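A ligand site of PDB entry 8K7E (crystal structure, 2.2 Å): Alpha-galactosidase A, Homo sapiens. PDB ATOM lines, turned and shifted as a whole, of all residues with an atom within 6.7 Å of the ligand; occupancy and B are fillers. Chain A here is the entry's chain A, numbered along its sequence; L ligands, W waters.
Water W3 lies within hydrogen-bond range of OD2 of Asp 235 (2.6 Å), O2 of the ligand (3.0 Å) and OD1 of Asp 200 (3.4 Å).
The side-chain carboxylate of Asp 139 sits at hydrogen-bond distance from the side-chain hydroxyl of Tyr 103 (2.5 Å).
The side-chain carboxylate of Asp 200 is in salt-bridge range of the guanidinium group of Arg 196 (2.9 Å).
OE2 of Glu 172 lies within salt-bridge range of NZ of Lys 137 (3.8 Å).
OD2 of Asp 61 lies within salt-bridge range of NZ of Lys 137, 2.8 Å away.
OD2 of Asp 62 is in hydrogen-bond range of N of Ala 112, 2.9 Å away.
OD2 of Asp 235 is in salt-bridge range of NH1 of Arg 196, 3.5 Å away.
The backbone carbonyl oxygen (O) of Phe 198 sits at hydrogen-bond distance from the guanidinium group (NH2) of Arg 196, at 2.7 Å.
OH of Tyr 176 is in hydrogen-bond range of SG of Cys 141 (3.6 Å).
N1 of the ligand lies within salt-bridge range of OD2 of Asp 139, 2.5 Å away.
The side-chain carboxylate (OD1) of Asp 200 is in salt-bridge range of a nitrogen (N2) of the ligand, at 2.5 Å.
The side-chain carboxylate of Glu 172 is in salt-bridge range of a nitrogen (N2) of the ligand, at 2.6 Å.
The side-chain carboxylate (OD1) of Asp 61 sits at hydrogen-bond distance from an oxygen (O1) of the ligand.
The side-chain carboxylate (OD2) of Asp 62 is in hydrogen-bond range of an oxygen (O3) of the ligand (2.9 Å).
The side-chain amino group (NZ) of Lys 137 sits at hydrogen-bond distance from an oxygen (O1) of the ligand.
The guanidinium group of Arg 196 sits at hydrogen-bond distance from an oxygen (O2) of the ligand, 3.2 Å away.
The side-chain sulfur (SG) of Cys 111 lies within hydrogen-bond range of a nitrogen (N1) of the ligand (3.4 Å).
Residues that only touch the ligand: Trp 16 (3.7 Å), Tyr 103 (3.6 Å), Ala 112 (3.9 Å), Leu 175 (3.7 Å) and Tyr 176 (3.3 Å).
Of the 25 residues printed, 13 come within 4 Å of the ligand.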
ATOM      1  N   LEU A  14      -6.082  -3.376  -4.520  1.00  0.00           N
ATOM      2  CA  LEU A  14      -4.780  -2.779  -4.227  1.00  0.00           C
ATOM      3  C   LEU A  14      -4.581  -2.840  -2.726  1.00  0.00           C
ATOM      4  O   LEU A  14      -5.482  -2.489  -1.961  1.00  0.00           O
ATOM      5  CB  LEU A  14      -4.752  -1.338  -4.743  1.00  0.00           C
ATOM      6  CG  LEU A  14      -3.500  -0.468  -4.559  1.00  0.00           C
ATOM      7  CD1 LEU A  14      -2.304  -1.090  -5.253  1.00  0.00           C
ATOM      8  CD2 LEU A  14      -3.792   0.925  -5.113  1.00  0.00           C
ATOM      9  N   TRP A  16      -2.712  -1.223  -0.471  1.00  0.00           N
ATOM     10  CA  TRP A  16      -2.076  -0.195   0.353  1.00  0.00           C
ATOM     11  C   TRP A  16      -2.896   0.167   1.583  1.00  0.00           C
ATOM     12  O   TRP A  16      -2.393   0.120   2.710  1.00  0.00           O
ATOM     13  CB  TRP A  16      -1.767   1.061  -0.454  1.00  0.00           C
ATOM     14  CG  TRP A  16      -1.041   2.022   0.419  1.00  0.00           C
ATOM     15  CD1 TRP A  16      -1.508   3.214   0.900  1.00  0.00           C
ATOM     16  CD2 TRP A  16       0.257   1.848   0.986  1.00  0.00           C
ATOM     17  NE1 TRP A  16      -0.563   3.802   1.696  1.00  0.00           N
ATOM     18  CE2 TRP A  16       0.537   2.982   1.772  1.00  0.00           C
ATOM     19  CE3 TRP A  16       1.232   0.839   0.898  1.00  0.00           C
ATOM     20  CZ2 TRP A  16       1.736   3.131   2.469  1.00  0.00           C
ATOM     21  CZ3 TRP A  16       2.425   1.004   1.590  1.00  0.00           C
ATOM     22  CH2 TRP A  16       2.669   2.135   2.365  1.00  0.00           C
ATOM     23  N   CYS A  21       2.455  -1.053   4.777  1.00  0.00           N
ATOM     24  CA  CYS A  21       3.826  -1.514   4.625  1.00  0.00           C
ATOM     25  C   CYS A  21       4.192  -2.470   5.753  1.00  0.00           C
ATOM     26  O   CYS A  21       5.209  -2.276   6.428  1.00  0.00           O
ATOM     27  CB  CYS A  21       4.793  -0.340   4.582  1.00  0.00           C
ATOM     28  SG  CYS A  21       6.455  -0.789   4.046  1.00  0.00           S
ATOM     29  N   ASP A  61       1.168  -2.794  -4.161  1.00  0.00           N
ATOM     30  CA  ASP A  61       1.597  -1.422  -3.912  1.00  0.00           C
ATOM     31  C   ASP A  61       3.025  -1.454  -3.366  1.00  0.00           C
ATOM     32  O   ASP A  61       3.780  -2.406  -3.608  1.00  0.00           O
ATOM     33  CB  ASP A  61       0.598  -0.741  -2.963  1.00  0.00           C
ATOM     34  CG  ASP A  61       0.522   0.760  -3.193  1.00  0.00           C
ATOM     35  OD1 ASP A  61       1.463   1.479  -2.806  1.00  0.00           O
ATOM     36  OD2 ASP A  61      -0.499   1.222  -3.768  1.00  0.00           O
ATOM     37  N   ASP A  62       3.413  -0.416  -2.615  1.00  0.00           N
ATOM     38  CA  ASP A  62       4.786  -0.289  -2.131  1.00  0.00           C
ATOM     39  C   ASP A  62       5.129  -1.405  -1.150  1.00  0.00           C
ATOM     40  O   ASP A  62       4.255  -2.110  -0.629  1.00  0.00           O
ATOM     41  CB  ASP A  62       4.965   1.080  -1.476  1.00  0.00           C
ATOM     42  CG  ASP A  62       6.423   1.511  -1.357  1.00  0.00           C
ATOM     43  OD1 ASP A  62       7.329   0.708  -1.639  1.00  0.00           O
ATOM     44  OD2 ASP A  62       6.651   2.686  -0.988  1.00  0.00           O
ATOM     45  N   CYS A  63       6.428  -1.577  -0.920  1.00  0.00           N
ATOM     46  CA  CYS A  63       7.003  -2.538   0.031  1.00  0.00           C
ATOM     47  C   CYS A  63       6.961  -3.985  -0.465  1.00  0.00           C
ATOM     48  O   CYS A  63       6.797  -4.907   0.342  1.00  0.00           O
ATOM     49  CB  CYS A  63       6.329  -2.414   1.409  1.00  0.00           C
ATOM     50  SG  CYS A  63       6.334  -0.699   2.015  1.00  0.00           S
ATOM     51  N   TYR A 103       4.226  -1.818  -8.473  1.00  0.00           N
ATOM     52  CA  TYR A 103       4.448  -0.454  -8.010  1.00  0.00           C
ATOM     53  C   TYR A 103       5.901  -0.070  -8.202  1.00  0.00           C
ATOM     54  O   TYR A 103       6.809  -0.884  -7.981  1.00  0.00           O
ATOM     55  CB  TYR A 103       4.034  -0.323  -6.522  1.00  0.00           C
ATOM     56  CG  TYR A 103       4.475   0.944  -5.813  1.00  0.00           C
ATOM     57  CD1 TYR A 103       5.779   1.097  -5.350  1.00  0.00           C
ATOM     58  CD2 TYR A 103       3.580   1.985  -5.580  1.00  0.00           C
ATOM     59  CE1 TYR A 103       6.186   2.249  -4.698  1.00  0.00           C
ATOM     60  CE2 TYR A 103       3.969   3.142  -4.916  1.00  0.00           C
ATOM     61  CZ  TYR A 103       5.279   3.268  -4.483  1.00  0.00           C
ATOM     62  OH  TYR A 103       5.691   4.405  -3.827  1.00  0.00           O
ATOM     63  N   ASP A 105       8.495   3.944  -8.361  1.00  0.00           N
ATOM     64  CA  ASP A 105       8.532   5.365  -8.031  1.00  0.00           C
ATOM     65  C   ASP A 105       9.425   6.132  -8.997  1.00  0.00           C
ATOM     66  O   ASP A 105      10.520   5.685  -9.335  1.00  0.00           O
ATOM     67  CB  ASP A 105       9.020   5.559  -6.592  1.00  0.00           C
ATOM     68  CG  ASP A 105       8.765   6.958  -6.061  1.00  0.00           C
ATOM     69  OD1 ASP A 105       9.423   7.914  -6.525  1.00  0.00           O
ATOM     70  OD2 ASP A 105       7.904   7.114  -5.172  1.00  0.00           O
ATOM     71  N   THR A 110      11.239   4.837  -3.370  1.00  0.00           N
ATOM     72  CA  THR A 110       9.802   4.785  -3.164  1.00  0.00           C
ATOM     73  C   THR A 110       9.448   5.523  -1.878  1.00  0.00           C
ATOM     74  O   THR A 110      10.305   5.861  -1.066  1.00  0.00           O
ATOM     75  CB  THR A 110       9.309   3.340  -3.087  1.00  0.00           C
ATOM     76  OG1 THR A 110       9.648   2.772  -1.810  1.00  0.00           O
ATOM     77  CG2 THR A 110       9.909   2.491  -4.196  1.00  0.00           C
ATOM     78  N   CYS A 111       8.147   5.797  -1.706  1.00  0.00           N
ATOM     79  CA  CYS A 111       7.724   6.545  -0.530  1.00  0.00           C
ATOM     80  C   CYS A 111       8.108   5.834   0.772  1.00  0.00           C
ATOM     81  O   CYS A 111       8.383   6.491   1.770  1.00  0.00           O
ATOM     82  CB  CYS A 111       6.224   6.817  -0.574  1.00  0.00           C
ATOM     83  SG  CYS A 111       5.723   7.954  -1.901  1.00  0.00           S
ATOM     84  N   ALA A 112       8.140   4.507   0.766  1.00  0.00           N
ATOM     85  CA  ALA A 112       8.565   3.761   1.940  1.00  0.00           C
ATOM     86  C   ALA A 112      10.071   3.546   2.013  1.00  0.00           C
ATOM     87  O   ALA A 112      10.542   2.898   2.954  1.00  0.00           O
ATOM     88  CB  ALA A 112       7.842   2.409   1.981  1.00  0.00           C
ATOM     89  N   GLY A 113      10.841   4.056   1.062  1.00  0.00           N
ATOM     90  CA  GLY A 113      12.286   4.032   1.157  1.00  0.00           C
ATOM     91  C   GLY A 113      12.982   2.931   0.384  1.00  0.00           C
ATOM     92  O   GLY A 113      14.188   2.728   0.596  1.00  0.00           O
ATOM     93  N   LYS A 137       1.584   1.152 -11.080  1.00  0.00           N
ATOM     94  CA  LYS A 137       1.326   2.359 -10.296  1.00  0.00           C
ATOM     95  C   LYS A 137       2.664   3.025 -10.023  1.00  0.00           C
ATOM     96  O   LYS A 137       3.558   2.424  -9.405  1.00  0.00           O
ATOM     97  CB  LYS A 137       0.611   2.032  -8.991  1.00  0.00           C
ATOM     98  CG  LYS A 137       0.214   3.255  -8.165  1.00  0.00           C
ATOM     99  CD  LYS A 137      -0.376   2.868  -6.811  1.00  0.00           C
ATOM    100  CE  LYS A 137      -0.366   4.044  -5.845  1.00  0.00           C
ATOM    101  NZ  LYS A 137      -1.156   3.775  -4.614  1.00  0.00           N
ATOM    102  N   ASP A 139       4.677   6.063  -8.389  1.00  0.00           N
ATOM    103  CA  ASP A 139       4.615   7.045  -7.317  1.00  0.00           C
ATOM    104  C   ASP A 139       5.595   8.195  -7.558  1.00  0.00           C
ATOM    105  O   ASP A 139       6.487   8.124  -8.398  1.00  0.00           O
ATOM    106  CB  ASP A 139       4.900   6.350  -5.995  1.00  0.00           C
ATOM    107  CG  ASP A 139       4.158   6.961  -4.834  1.00  0.00           C
ATOM    108  OD1 ASP A 139       3.610   8.061  -4.961  1.00  0.00           O
ATOM    109  OD2 ASP A 139       4.107   6.297  -3.777  1.00  0.00           O
ATOM    110  N   GLY A 140       5.435   9.271  -6.788  1.00  0.00           N
ATOM    111  CA  GLY A 140       6.224  10.475  -6.995  1.00  0.00           C
ATOM    112  C   GLY A 140       7.130  10.942  -5.869  1.00  0.00           C
ATOM    113  O   GLY A 140       7.534  12.103  -5.857  1.00  0.00           O
ATOM    114  N   CYS A 141       7.471  10.074  -4.911  1.00  0.00           N
ATOM    115  CA  CYS A 141       8.291  10.491  -3.788  1.00  0.00           C
ATOM    116  C   CYS A 141       9.761  10.623  -4.190  1.00  0.00           C
ATOM    117  O   CYS A 141      10.218  10.017  -5.172  1.00  0.00           O
ATOM    118  CB  CYS A 141       8.198   9.493  -2.629  1.00  0.00           C
ATOM    119  SG  CYS A 141       6.774   9.666  -1.559  1.00  0.00           S
ATOM    120  N   GLU A 172       0.796   9.204 -10.259  1.00  0.00           N
ATOM    121  CA  GLU A 172       0.512  10.151  -9.191  1.00  0.00           C
ATOM    122  C   GLU A 172       1.046  11.550  -9.506  1.00  0.00           C
ATOM    123  O   GLU A 172       1.079  12.411  -8.623  1.00  0.00           O
ATOM    124  CB  GLU A 172       1.090   9.640  -7.860  1.00  0.00           C
ATOM    125  CG  GLU A 172       0.500   8.313  -7.405  1.00  0.00           C
ATOM    126  CD  GLU A 172       0.502   8.164  -5.885  1.00  0.00           C
ATOM    127  OE1 GLU A 172       0.363   9.179  -5.167  1.00  0.00           O
ATOM    128  OE2 GLU A 172       0.618   7.015  -5.413  1.00  0.00           O
ATOM    129  N   LEU A 175      -0.879  14.864  -8.366  1.00  0.00           N
ATOM    130  CA  LEU A 175      -0.825  15.036  -6.921  1.00  0.00           C
ATOM    131  C   LEU A 175       0.496  15.644  -6.477  1.00  0.00           C
ATOM    132  O   LEU A 175       0.523  16.524  -5.609  1.00  0.00           O
ATOM    133  CB  LEU A 175      -1.049  13.686  -6.232  1.00  0.00           C
ATOM    134  CG  LEU A 175      -0.806  13.646  -4.714  1.00  0.00           C
ATOM    135  CD1 LEU A 175      -1.740  14.611  -4.000  1.00  0.00           C
ATOM    136  CD2 LEU A 175      -0.964  12.223  -4.177  1.00  0.00           C
ATOM    137  N   TYR A 176       1.615  15.197  -7.069  1.00  0.00           N
ATOM    138  CA  TYR A 176       2.904  15.735  -6.647  1.00  0.00           C
ATOM    139  C   TYR A 176       3.214  17.072  -7.312  1.00  0.00           C
ATOM    140  O   TYR A 176       4.117  17.772  -6.846  1.00  0.00           O
ATOM    141  CB  TYR A 176       4.016  14.718  -6.943  1.00  0.00           C
ATOM    142  CG  TYR A 176       3.967  13.555  -5.976  1.00  0.00           C
ATOM    143  CD1 TYR A 176       3.107  12.487  -6.206  1.00  0.00           C
ATOM    144  CD2 TYR A 176       4.765  13.532  -4.839  1.00  0.00           C
ATOM    145  CE1 TYR A 176       3.042  11.426  -5.321  1.00  0.00           C
ATOM    146  CE2 TYR A 176       4.709  12.467  -3.955  1.00  0.00           C
ATOM    147  CZ  TYR A 176       3.843  11.418  -4.200  1.00  0.00           C
ATOM    148  OH  TYR A 176       3.778  10.363  -3.334  1.00  0.00           O
ATOM    149  N   ARG A 196      -3.677  10.143  -9.982  1.00  0.00           N
ATOM    150  CA  ARG A 196      -4.091  10.552  -8.655  1.00  0.00           C
ATOM    151  C   ARG A 196      -4.057  12.076  -8.534  1.00  0.00           C
ATOM    152  O   ARG A 196      -3.032  12.703  -8.811  1.00  0.00           O
ATOM    153  CB  ARG A 196      -3.185   9.911  -7.598  1.00  0.00           C
ATOM    154  CG  ARG A 196      -3.427   8.412  -7.389  1.00  0.00           C
ATOM    155  CD  ARG A 196      -4.622   8.185  -6.469  1.00  0.00           C
ATOM    156  NE  ARG A 196      -4.528   9.051  -5.291  1.00  0.00           N
ATOM    157  CZ  ARG A 196      -3.724   8.819  -4.265  1.00  0.00           C
ATOM    158  NH1 ARG A 196      -3.010   7.713  -4.177  1.00  0.00           N
ATOM    159  NH2 ARG A 196      -3.635   9.733  -3.304  1.00  0.00           N
ATOM    160  N   PHE A 198      -5.369  13.829  -5.536  1.00  0.00           N
ATOM    161  CA  PHE A 198      -5.571  14.353  -4.188  1.00  0.00           C
ATOM    162  C   PHE A 198      -4.942  13.412  -3.159  1.00  0.00           C
ATOM    163  O   PHE A 198      -4.528  12.295  -3.476  1.00  0.00           O
ATOM    164  CB  PHE A 198      -7.076  14.539  -3.913  1.00  0.00           C
ATOM    165  CG  PHE A 198      -7.389  15.271  -2.630  1.00  0.00           C
ATOM    166  CD1 PHE A 198      -7.034  16.600  -2.466  1.00  0.00           C
ATOM    167  CD2 PHE A 198      -8.028  14.614  -1.584  1.00  0.00           C
ATOM    168  CE1 PHE A 198      -7.313  17.267  -1.280  1.00  0.00           C
ATOM    169  CE2 PHE A 198      -8.316  15.267  -0.412  1.00  0.00           C
ATOM    170  CZ  PHE A 198      -7.957  16.605  -0.246  1.00  0.00           C
ATOM    171  N   ALA A 199      -4.896  13.891  -1.918  1.00  0.00           N
ATOM    172  CA  ALA A 199      -4.237  13.189  -0.821  1.00  0.00           C
ATOM    173  C   ALA A 199      -4.771  11.766  -0.651  1.00  0.00           C
ATOM    174  O   ALA A 199      -5.925  11.465  -0.968  1.00  0.00           O
ATOM    175  CB  ALA A 199      -4.418  13.968   0.484  1.00  0.00           C
ATOM    176  N   ASP A 200      -3.896  10.890  -0.145  1.00  0.00           N
ATOM    177  CA  ASP A 200      -4.238   9.483   0.098  1.00  0.00           C
ATOM    178  C   ASP A 200      -5.525   9.345   0.903  1.00  0.00           C
ATOM    179  O   ASP A 200      -5.752  10.068   1.874  1.00  0.00           O
ATOM    180  CB  ASP A 200      -3.112   8.779   0.853  1.00  0.00           C
ATOM    181  CG  ASP A 200      -1.812   8.716   0.087  1.00  0.00           C
ATOM    182  OD1 ASP A 200      -1.798   9.003  -1.136  1.00  0.00           O
ATOM    183  OD2 ASP A 200      -0.785   8.362   0.708  1.00  0.00           O
ATOM    184  N   ASP A 235      -8.668   7.669  -5.598  1.00  0.00           N
ATOM    185  CA  ASP A 235      -8.060   6.679  -4.710  1.00  0.00           C
ATOM    186  C   ASP A 235      -9.018   5.544  -4.370  1.00  0.00           C
ATOM    187  O   ASP A 235     -10.135   5.474  -4.896  1.00  0.00           O
ATOM    188  CB  ASP A 235      -7.508   7.316  -3.433  1.00  0.00           C
ATOM    189  CG  ASP A 235      -6.243   6.637  -2.958  1.00  0.00           C
ATOM    190  OD1 ASP A 235      -5.872   5.605  -3.551  1.00  0.00           O
ATOM    191  OD2 ASP A 235      -5.622   7.136  -1.991  1.00  0.00           O
ATOM    192  N   MET A 236      -8.574   4.663  -3.483  1.00  0.00           N
ATOM    193  CA  MET A 236      -9.150   3.323  -3.370  1.00  0.00           C
ATOM    194  C   MET A 236     -10.533   3.339  -2.732  1.00  0.00           C
ATOM    195  O   MET A 236     -10.878   4.217  -1.938  1.00  0.00           O
ATOM    196  CB  MET A 236      -8.225   2.419  -2.558  1.00  0.00           C
ATOM    197  CG  MET A 236      -6.821   2.292  -3.127  1.00  0.00           C
ATOM    198  SD  MET A 236      -5.639   1.719  -1.888  1.00  0.00           S
ATOM    199  CE  MET A 236      -4.931   3.270  -1.378  1.00  0.00           C
HETATM  200  C1  LIG L   1       0.930   4.774  -1.579  1.00  0.00           C
HETATM  201  C2  LIG L   1       3.225   3.972  -1.039  1.00  0.00           C
HETATM  202  C3  LIG L   1       0.324   6.156  -1.685  1.00  0.00           C
HETATM  203  C4  LIG L   1       1.508   6.910  -2.305  1.00  0.00           C
HETATM  204  C5  LIG L   1       1.477   8.422  -2.017  1.00  0.00           C
HETATM  205  C6  LIG L   1       2.232   5.137  -0.910  1.00  0.00           C
HETATM  206  N1  LIG L   1       2.704   6.299  -1.690  1.00  0.00           N
HETATM  207  N2  LIG L   1       0.296   9.098  -2.569  1.00  0.00           N
HETATM  208  O1  LIG L   1       1.227   4.230  -2.894  1.00  0.00           O
HETATM  209  O2  LIG L   1      -0.800   6.135  -2.574  1.00  0.00           O
HETATM  210  O3  LIG L   1       4.359   4.189  -0.170  1.00  0.00           O
HETATM  211  O   HOH W   1       1.311  11.723  -1.157  1.00  0.00           O
HETATM  212  O   HOH W   2       4.939   5.348   2.131  1.00  0.00           O
HETATM  213  O   HOH W   3      -3.388   5.983  -1.154  1.00  0.00           O
